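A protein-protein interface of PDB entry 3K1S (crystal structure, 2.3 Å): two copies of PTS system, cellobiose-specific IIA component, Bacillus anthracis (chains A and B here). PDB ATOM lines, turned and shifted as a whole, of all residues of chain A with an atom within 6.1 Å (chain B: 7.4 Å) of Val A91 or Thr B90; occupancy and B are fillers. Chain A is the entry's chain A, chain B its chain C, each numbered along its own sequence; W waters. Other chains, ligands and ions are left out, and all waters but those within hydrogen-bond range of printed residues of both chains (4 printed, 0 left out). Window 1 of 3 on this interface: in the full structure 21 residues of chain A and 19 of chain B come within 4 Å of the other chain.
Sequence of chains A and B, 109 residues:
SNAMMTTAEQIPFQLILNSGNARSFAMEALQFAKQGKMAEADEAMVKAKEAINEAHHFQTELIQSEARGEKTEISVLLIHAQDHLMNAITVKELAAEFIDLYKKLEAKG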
ATOM      1  N   ARG A  23      17.003  33.128   4.885  1.00  0.00           N
ATOM      2  CA  ARG A  23      16.328  31.878   4.722  1.00  0.00           C
ATOM      3  C   ARG A  23      16.837  31.144   3.478  1.00  0.00           C
ATOM      4  O   ARG A  23      17.106  29.979   3.530  1.00  0.00           O
ATOM      5  CB  ARG A  23      14.826  32.109   4.621  1.00  0.00           C
ATOM      6  CG  ARG A  23      14.025  30.871   4.575  1.00  0.00           C
ATOM      7  CD  ARG A  23      12.660  31.071   3.957  1.00  0.00           C
ATOM      8  NE  ARG A  23      12.187  29.805   3.427  1.00  0.00           N
ATOM      9  CZ  ARG A  23      12.332  29.417   2.164  1.00  0.00           C
ATOM     10  NH1 ARG A  23      12.901  30.218   1.281  1.00  0.00           N
ATOM     11  NH2 ARG A  23      11.903  28.228   1.781  1.00  0.00           N
ATOM     12  N   ALA A  26      20.242  29.565   4.176  1.00  0.00           N
ATOM     13  CA  ALA A  26      20.070  28.388   5.022  1.00  0.00           C
ATOM     14  C   ALA A  26      19.574  27.179   4.227  1.00  0.00           C
ATOM     15  O   ALA A  26      20.095  26.079   4.389  1.00  0.00           O
ATOM     16  CB  ALA A  26      19.141  28.698   6.196  1.00  0.00           C
ATOM     17  N   MET A  27      18.581  27.378   3.364  1.00  0.00           N
ATOM     18  CA  MET A  27      18.059  26.276   2.549  1.00  0.00           C
ATOM     19  C   MET A  27      19.081  25.815   1.499  1.00  0.00           C
ATOM     20  O   MET A  27      19.210  24.618   1.236  1.00  0.00           O
ATOM     21  CB  MET A  27      16.721  26.642   1.889  1.00  0.00           C
ATOM     22  CG  MET A  27      15.566  26.862   2.866  1.00  0.00           C
ATOM     23  SD  MET A  27      15.221  25.403   4.149  1.00  0.00           S
ATOM     24  CE  MET A  27      14.852  23.949   2.888  1.00  0.00           C
ATOM     25  N   MET A  45      25.926  28.726   5.469  1.00  0.00           N
ATOM     26  CA  MET A  45      25.460  29.004   6.829  1.00  0.00           C
ATOM     27  C   MET A  45      26.062  30.297   7.387  1.00  0.00           C
ATOM     28  O   MET A  45      25.379  31.068   8.070  1.00  0.00           O
ATOM     29  CB  MET A  45      25.743  27.819   7.761  1.00  0.00           C
ATOM     30  CG  MET A  45      24.841  26.617   7.494  1.00  0.00           C
ATOM     31  SD  MET A  45      22.934  27.022   7.775  1.00  0.00           S
ATOM     32  CE  MET A  45      22.979  27.111   9.735  1.00  0.00           C
ATOM     33  N   MET A  86      11.825  36.362  12.105  1.00  0.00           N
ATOM     34  CA  MET A  86      11.776  35.267  13.068  1.00  0.00           C
ATOM     35  C   MET A  86      11.800  33.888  12.397  1.00  0.00           C
ATOM     36  O   MET A  86      12.393  32.949  12.934  1.00  0.00           O
ATOM     37  CB  MET A  86      10.565  35.409  14.005  1.00  0.00           C
ATOM     38  CG  MET A  86      10.692  36.587  14.968  1.00  0.00           C
ATOM     39  SD  MET A  86      12.230  36.421  16.190  1.00  0.00           S
ATOM     40  CE  MET A  86      11.441  35.172  17.478  1.00  0.00           C
ATOM     41  N   ASN A  87      11.170  33.776  11.228  1.00  0.00           N
ATOM     42  CA  ASN A  87      11.213  32.544  10.435  1.00  0.00           C
ATOM     43  C   ASN A  87      12.615  32.186   9.933  1.00  0.00           C
ATOM     44  O   ASN A  87      13.023  31.025   9.990  1.00  0.00           O
ATOM     45  CB  ASN A  87      10.250  32.613   9.242  1.00  0.00           C
ATOM     46  CG  ASN A  87      10.110  31.273   8.546  1.00  0.00           C
ATOM     47  OD1 ASN A  87       9.771  30.276   9.176  1.00  0.00           O
ATOM     48  ND2 ASN A  87      10.393  31.241   7.249  1.00  0.00           N
ATOM     49  N   ALA A  88      13.336  33.188   9.436  1.00  0.00           N
ATOM     50  CA  ALA A  88      14.715  33.011   8.968  1.00  0.00           C
ATOM     51  C   ALA A  88      15.609  32.482  10.084  1.00  0.00           C
ATOM     52  O   ALA A  88      16.420  31.581   9.873  1.00  0.00           O
ATOM     53  CB  ALA A  88      15.259  34.331   8.423  1.00  0.00           C
ATOM     54  N   ILE A  89      15.449  33.044  11.276  1.00  0.00           N
ATOM     55  CA  ILE A  89      16.194  32.607  12.452  1.00  0.00           C
ATOM     56  C   ILE A  89      15.885  31.132  12.760  1.00  0.00           C
ATOM     57  O   ILE A  89      16.790  30.343  13.037  1.00  0.00           O
ATOM     58  CB  ILE A  89      15.893  33.532  13.673  1.00  0.00           C
ATOM     59  CG1 ILE A  89      16.490  34.927  13.442  1.00  0.00           C
ATOM     60  CG2 ILE A  89      16.418  32.938  14.966  1.00  0.00           C
ATOM     61  CD1 ILE A  89      15.933  36.032  14.361  1.00  0.00           C
ATOM     62  N   THR A  90      14.607  30.766  12.704  1.00  0.00           N
ATOM     63  CA  THR A  90      14.198  29.387  12.973  1.00  0.00           C
ATOM     64  C   THR A  90      14.738  28.428  11.917  1.00  0.00           C
ATOM     65  O   THR A  90      15.254  27.364  12.255  1.00  0.00           O
ATOM     66  CB  THR A  90      12.663  29.261  13.101  1.00  0.00           C
ATOM     67  OG1 THR A  90      12.241  29.940  14.289  1.00  0.00           O
ATOM     68  CG2 THR A  90      12.236  27.799  13.186  1.00  0.00           C
ATOM     69  N   VAL A  91      14.626  28.812  10.649  1.00  0.00           N
ATOM     70  CA  VAL A  91      15.099  27.976   9.541  1.00  0.00           C
ATOM     71  C   VAL A  91      16.618  27.767   9.591  1.00  0.00           C
ATOM     72  O   VAL A  91      17.097  26.654   9.403  1.00  0.00           O
ATOM     73  CB  VAL A  91      14.649  28.537   8.166  1.00  0.00           C
ATOM     74  CG1 VAL A  91      15.229  27.724   7.024  1.00  0.00           C
ATOM     75  CG2 VAL A  91      13.121  28.543   8.076  1.00  0.00           C
ATOM     76  N   LYS A  92      17.368  28.836   9.847  1.00  0.00           N
ATOM     77  CA  LYS A  92      18.811  28.728   9.997  1.00  0.00           C
ATOM     78  C   LYS A  92      19.170  27.769  11.134  1.00  0.00           C
ATOM     79  O   LYS A  92      20.017  26.886  10.968  1.00  0.00           O
ATOM     80  CB  LYS A  92      19.439  30.104  10.234  1.00  0.00           C
ATOM     81  CG  LYS A  92      20.950  30.073  10.414  1.00  0.00           C
ATOM     82  CD  LYS A  92      21.481  31.446  10.794  1.00  0.00           C
ATOM     83  CE  LYS A  92      22.903  31.368  11.308  1.00  0.00           C
ATOM     84  NZ  LYS A  92      22.982  30.705  12.641  1.00  0.00           N
ATOM     85  N   GLU A  93      18.514  27.944  12.279  1.00  0.00           N
ATOM     86  CA  GLU A  93      18.786  27.131  13.459  1.00  0.00           C
ATOM     87  C   GLU A  93      18.524  25.648  13.209  1.00  0.00           C
ATOM     88  O   GLU A  93      19.277  24.794  13.677  1.00  0.00           O
ATOM     89  CB  GLU A  93      17.970  27.628  14.662  1.00  0.00           C
ATOM     90  CG  GLU A  93      18.329  26.946  15.977  1.00  0.00           C
ATOM     91  CD  GLU A  93      17.759  27.643  17.204  1.00  0.00           C
ATOM     92  OE1 GLU A  93      16.757  28.380  17.079  1.00  0.00           O
ATOM     93  OE2 GLU A  93      18.318  27.439  18.305  1.00  0.00           O
ATOM     94  N   LEU A  94      17.459  25.337  12.482  1.00  0.00           N
ATOM     95  CA  LEU A  94      17.134  23.938  12.210  1.00  0.00           C
ATOM     96  C   LEU A  94      17.943  23.356  11.051  1.00  0.00           C
ATOM     97  O   LEU A  94      18.297  22.172  11.067  1.00  0.00           O
ATOM     98  CB  LEU A  94      15.633  23.758  11.998  1.00  0.00           C
ATOM     99  CG  LEU A  94      14.795  24.078  13.245  1.00  0.00           C
ATOM    100  CD1 LEU A  94      13.311  24.012  12.929  1.00  0.00           C
ATOM    101  CD2 LEU A  94      15.147  23.148  14.418  1.00  0.00           C
ATOM    102  N   ALA A  95      18.247  24.194  10.064  1.00  0.00           N
ATOM    103  CA  ALA A  95      19.066  23.781   8.933  1.00  0.00           C
ATOM    104  C   ALA A  95      20.458  23.353   9.408  1.00  0.00           C
ATOM    105  O   ALA A  95      21.036  22.405   8.875  1.00  0.00           O
ATOM    106  CB  ALA A  95      19.157  24.896   7.905  1.00  0.00           C
ATOM    107  N   ALA A  96      20.988  24.062  10.404  1.00  0.00           N
ATOM    108  CA  ALA A  96      22.205  23.652  11.104  1.00  0.00           C
ATOM    109  C   ALA A  96      22.098  22.211  11.591  1.00  0.00           C
ATOM    110  O   ALA A  96      23.065  21.442  11.522  1.00  0.00           O
ATOM    111  CB  ALA A  96      22.479  24.582  12.283  1.00  0.00           C
ATOM    112  N   ILE B  52      -2.518  24.545   2.771  1.00  0.00           N
ATOM    113  CA  ILE B  52      -1.611  25.705   2.749  1.00  0.00           C
ATOM    114  C   ILE B  52      -2.082  26.731   1.711  1.00  0.00           C
ATOM    115  O   ILE B  52      -2.104  27.932   1.973  1.00  0.00           O
ATOM    116  CB  ILE B  52      -0.132  25.285   2.462  1.00  0.00           C
ATOM    117  CG1 ILE B  52       0.550  24.746   3.731  1.00  0.00           C
ATOM    118  CG2 ILE B  52       0.673  26.435   1.831  1.00  0.00           C
ATOM    119  CD1 ILE B  52       0.891  25.785   4.801  1.00  0.00           C
ATOM    120  N   HIS B  84       0.400  31.444  12.490  1.00  0.00           N
ATOM    121  CA  HIS B  84       0.002  30.081  12.176  1.00  0.00           C
ATOM    122  C   HIS B  84       0.408  29.681  10.765  1.00  0.00           C
ATOM    123  O   HIS B  84       0.897  28.573  10.557  1.00  0.00           O
ATOM    124  CB  HIS B  84      -1.511  29.906  12.364  1.00  0.00           C
ATOM    125  CG  HIS B  84      -1.907  29.453  13.736  1.00  0.00           C
ATOM    126  ND1 HIS B  84      -1.770  28.147  14.157  1.00  0.00           N
ATOM    127  CD2 HIS B  84      -2.460  30.125  14.774  1.00  0.00           C
ATOM    128  CE1 HIS B  84      -2.207  28.037  15.399  1.00  0.00           C
ATOM    129  NE2 HIS B  84      -2.632  29.224  15.797  1.00  0.00           N
ATOM    130  N   LEU B  85       0.214  30.579   9.799  1.00  0.00           N
ATOM    131  CA  LEU B  85       0.617  30.302   8.420  1.00  0.00           C
ATOM    132  C   LEU B  85       2.135  30.229   8.248  1.00  0.00           C
ATOM    133  O   LEU B  85       2.643  29.268   7.665  1.00  0.00           O
ATOM    134  CB  LEU B  85       0.027  31.325   7.440  1.00  0.00           C
ATOM    135  CG  LEU B  85       0.450  31.130   5.980  1.00  0.00           C
ATOM    136  CD1 LEU B  85       0.031  29.746   5.465  1.00  0.00           C
ATOM    137  CD2 LEU B  85      -0.090  32.253   5.075  1.00  0.00           C
ATOM    138  N   MET B  86       2.849  31.245   8.732  1.00  0.00           N
ATOM    139  CA  MET B  86       4.307  31.285   8.598  1.00  0.00           C
ATOM    140  C   MET B  86       4.926  30.003   9.159  1.00  0.00           C
ATOM    141  O   MET B  86       5.789  29.412   8.535  1.00  0.00           O
ATOM    142  CB  MET B  86       4.885  32.519   9.297  1.00  0.00           C
ATOM    143  CG  MET B  86       6.390  32.717   9.125  1.00  0.00           C
ATOM    144  SD  MET B  86       6.932  33.180   7.296  1.00  0.00           S
ATOM    145  CE  MET B  86       7.183  31.367   6.598  1.00  0.00           C
ATOM    146  N   ASN B  87       4.464  29.574  10.330  1.00  0.00           N
ATOM    147  CA  ASN B  87       4.963  28.350  10.947  1.00  0.00           C
ATOM    148  C   ASN B  87       4.484  27.063  10.265  1.00  0.00           C
ATOM    149  O   ASN B  87       5.230  26.084  10.192  1.00  0.00           O
ATOM    150  CB  ASN B  87       4.645  28.335  12.446  1.00  0.00           C
ATOM    151  CG  ASN B  87       5.546  29.264  13.234  1.00  0.00           C
ATOM    152  OD1 ASN B  87       6.540  28.832  13.811  1.00  0.00           O
ATOM    153  ND2 ASN B  87       5.213  30.552  13.246  1.00  0.00           N
ATOM    154  N   ALA B  88       3.250  27.067   9.768  1.00  0.00           N
ATOM    155  CA  ALA B  88       2.732  25.935   8.997  1.00  0.00           C
ATOM    156  C   ALA B  88       3.567  25.725   7.734  1.00  0.00           C
ATOM    157  O   ALA B  88       3.957  24.603   7.419  1.00  0.00           O
ATOM    158  CB  ALA B  88       1.248  26.139   8.648  1.00  0.00           C
ATOM    159  N   ILE B  89       3.849  26.807   7.019  1.00  0.00           N
ATOM    160  CA  ILE B  89       4.703  26.745   5.828  1.00  0.00           C
ATOM    161  C   ILE B  89       6.065  26.123   6.154  1.00  0.00           C
ATOM    162  O   ILE B  89       6.545  25.241   5.438  1.00  0.00           O
ATOM    163  CB  ILE B  89       4.914  28.147   5.198  1.00  0.00           C
ATOM    164  CG1 ILE B  89       3.590  28.696   4.649  1.00  0.00           C
ATOM    165  CG2 ILE B  89       6.003  28.102   4.100  1.00  0.00           C
ATOM    166  CD1 ILE B  89       3.652  30.169   4.215  1.00  0.00           C
ATOM    167  N   THR B  90       6.686  26.585   7.233  1.00  0.00           N
ATOM    168  CA  THR B  90       8.017  26.105   7.594  1.00  0.00           C
ATOM    169  C   THR B  90       8.001  24.648   8.067  1.00  0.00           C
ATOM    170  O   THR B  90       8.920  23.887   7.771  1.00  0.00           O
ATOM    171  CB  THR B  90       8.688  27.037   8.623  1.00  0.00           C
ATOM    172  OG1 THR B  90       8.968  28.286   7.987  1.00  0.00           O
ATOM    173  CG2 THR B  90       9.997  26.442   9.144  1.00  0.00           C
ATOM    174  N   VAL B  91       6.955  24.271   8.798  1.00  0.00           N
ATOM    175  CA  VAL B  91       6.798  22.890   9.256  1.00  0.00           C
ATOM    176  C   VAL B  91       6.628  21.958   8.050  1.00  0.00           C
ATOM    177  O   VAL B  91       7.329  20.946   7.935  1.00  0.00           O
ATOM    178  CB  VAL B  91       5.635  22.750  10.272  1.00  0.00           C
ATOM    179  CG1 VAL B  91       5.375  21.283  10.624  1.00  0.00           C
ATOM    180  CG2 VAL B  91       5.941  23.555  11.539  1.00  0.00           C
ATOM    181  N   LYS B  92       5.723  22.314   7.142  1.00  0.00           N
ATOM    182  CA  LYS B  92       5.566  21.573   5.890  1.00  0.00           C
ATOM    183  C   LYS B  92       6.901  21.414   5.152  1.00  0.00           C
ATOM    184  O   LYS B  92       7.256  20.312   4.730  1.00  0.00           O
ATOM    185  CB  LYS B  92       4.530  22.249   4.984  1.00  0.00           C
ATOM    186  CG  LYS B  92       4.247  21.482   3.701  1.00  0.00           C
ATOM    187  CD  LYS B  92       3.238  22.221   2.827  1.00  0.00           C
ATOM    188  CE  LYS B  92       3.085  21.562   1.460  1.00  0.00           C
ATOM    189  NZ  LYS B  92       4.316  21.706   0.637  1.00  0.00           N
ATOM    190  N   GLU B  93       7.637  22.496   5.001  1.00  0.00           N
ATOM    191  CA  GLU B  93       8.895  22.466   4.273  1.00  0.00           C
ATOM    192  C   GLU B  93       9.949  21.561   4.887  1.00  0.00           C
ATOM    193  O   GLU B  93      10.623  20.846   4.195  1.00  0.00           O
ATOM    194  CB  GLU B  93       9.458  23.867   4.189  1.00  0.00           C
ATOM    195  CG  GLU B  93      10.109  24.173   2.904  1.00  0.00           C
ATOM    196  CD  GLU B  93      10.285  25.647   2.696  1.00  0.00           C
ATOM    197  OE1 GLU B  93       9.593  26.422   3.358  1.00  0.00           O
ATOM    198  OE2 GLU B  93      11.104  26.045   1.864  1.00  0.00           O
ATOM    199  N   LEU B  94      10.064  21.602   6.198  1.00  0.00           N
ATOM    200  CA  LEU B  94      11.053  20.802   6.911  1.00  0.00           C
ATOM    201  C   LEU B  94      10.570  19.377   7.167  1.00  0.00           C
ATOM    202  O   LEU B  94      11.376  18.452   7.287  1.00  0.00           O
ATOM    203  CB  LEU B  94      11.478  21.494   8.212  1.00  0.00           C
ATOM    204  CG  LEU B  94      12.018  22.920   8.039  1.00  0.00           C
ATOM    205  CD1 LEU B  94      12.464  23.503   9.378  1.00  0.00           C
ATOM    206  CD2 LEU B  94      13.156  22.979   7.012  1.00  0.00           C
ATOM    207  N   ALA B  95       9.257  19.195   7.242  1.00  0.00           N
ATOM    208  CA  ALA B  95       8.706  17.850   7.279  1.00  0.00           C
ATOM    209  C   ALA B  95       9.119  17.115   6.003  1.00  0.00           C
ATOM    210  O   ALA B  95       9.418  15.920   6.041  1.00  0.00           O
ATOM    211  CB  ALA B  95       7.193  17.885   7.428  1.00  0.00           C
ATOM    212  N   ALA B  96       9.157  17.842   4.886  1.00  0.00           N
ATOM    213  CA  ALA B  96       9.588  17.281   3.596  1.00  0.00           C
ATOM    214  C   ALA B  96      11.049  16.856   3.632  1.00  0.00           C
ATOM    215  O   ALA B  96      11.421  15.843   3.037  1.00  0.00           O
ATOM    216  CB  ALA B  96       9.349  18.277   2.451  1.00  0.00           C
HETATM  217  O   HOH W   1       8.379  30.859  11.637  1.00  0.00           O
HETATM  218  O   HOH W   2      13.658  26.878  -0.209  1.00  0.00           O
HETATM  219  O   HOH W   3      10.897  28.612   5.293  1.00  0.00           O
HETATM  220  O   HOH W   4       8.554  28.661   1.580  1.00  0.00           O
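OE1 of Glu B93 is in salt-bridge range of NH2 of Arg A23 (3.3 Å).
OG1 of Thr B90 sits at hydrogen-bond distance from OD1 of Asn A87 (2.5 Å).
The backbone carbonyl oxygen of Met B86 sits at hydrogen-bond distance from the side-chain hydroxyl of Thr B90, 3.4 Å away.
Among the printed residues, merely in contact across the chains: Asn A87 with Met B86, Leu A94 with Leu B94 and Val A91 with Thr B90.
Printed residues of chain B within 4 Å of Arg A23: Glu B93 (2.3 Å).
Printed residues of chain B within 4 Å of Asn A87: Met B86 and Thr B90.
Of the printed residues of chain B, Val A91 touches Thr B90 (3.9 Å).
Printed residues of chain A within 4 Å of Met B86: Asn A87 (3.3 Å).
Thr B90 touches two residues of chain A.
Of the printed residues of chain A, Glu B93 touches Arg A23 (2.3 Å).
Of the printed residues of chain A, Leu B94 touches Leu A94.
The nearest residue of chain B that does not touch Val A91 is Leu B94 (5.2 Å).
The nearest printed residue of chain B that does not touch Arg A23 is Thr B90 (5.8 Å).
Printed residues of chain A that touch a printed residue of chain B: Arg A23, Asn A87, Val A91 and Leu A94.
Asn A87 touches Met B86, but with the chains exchanged Met A86 does not touch Asn B87 (7.2 Å).
Asn A87 touches Thr B90, but with the chains exchanged Thr A90 does not touch Asn B87 (5.8 Å).
Val A91 touches Thr B90, but with the chains exchanged Thr A90 does not touch Val B91 (7.7 Å).
Leu B94 touches its own counterpart, Leu A94.
Positions printed for both chains: 86, 87, 88, 89, 90, 91, 92, 93, 94, 95 and 96.
Of the 5 pairs that touch across the chains among the printed residues, 1 has its exchanged pair printed and touching as well.
Water W3 lies within hydrogen-bond range of the guanidinium group of Arg A23, the side-chain carboxylate of Glu B93, the side-chain amide nitrogen of Asn A87 and the side-chain hydroxyl of Thr B90.
Water W1 lies within hydrogen-bond range of the side-chain amide oxygen of Asn A87 (2.9 Å) and the side-chain amide oxygen of Asn B87 (3.5 Å).
Water W2 bridges the guanidinium group of Arg A23 (3.0 Å) and the side-chain carboxylate of Glu B93 (3.4 Å).
Water W4 lies within hydrogen-bond range of the side-chain carboxylate of Glu B93 (3.0 Å) and the guanidinium group of Arg A23 (3.4 Å).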
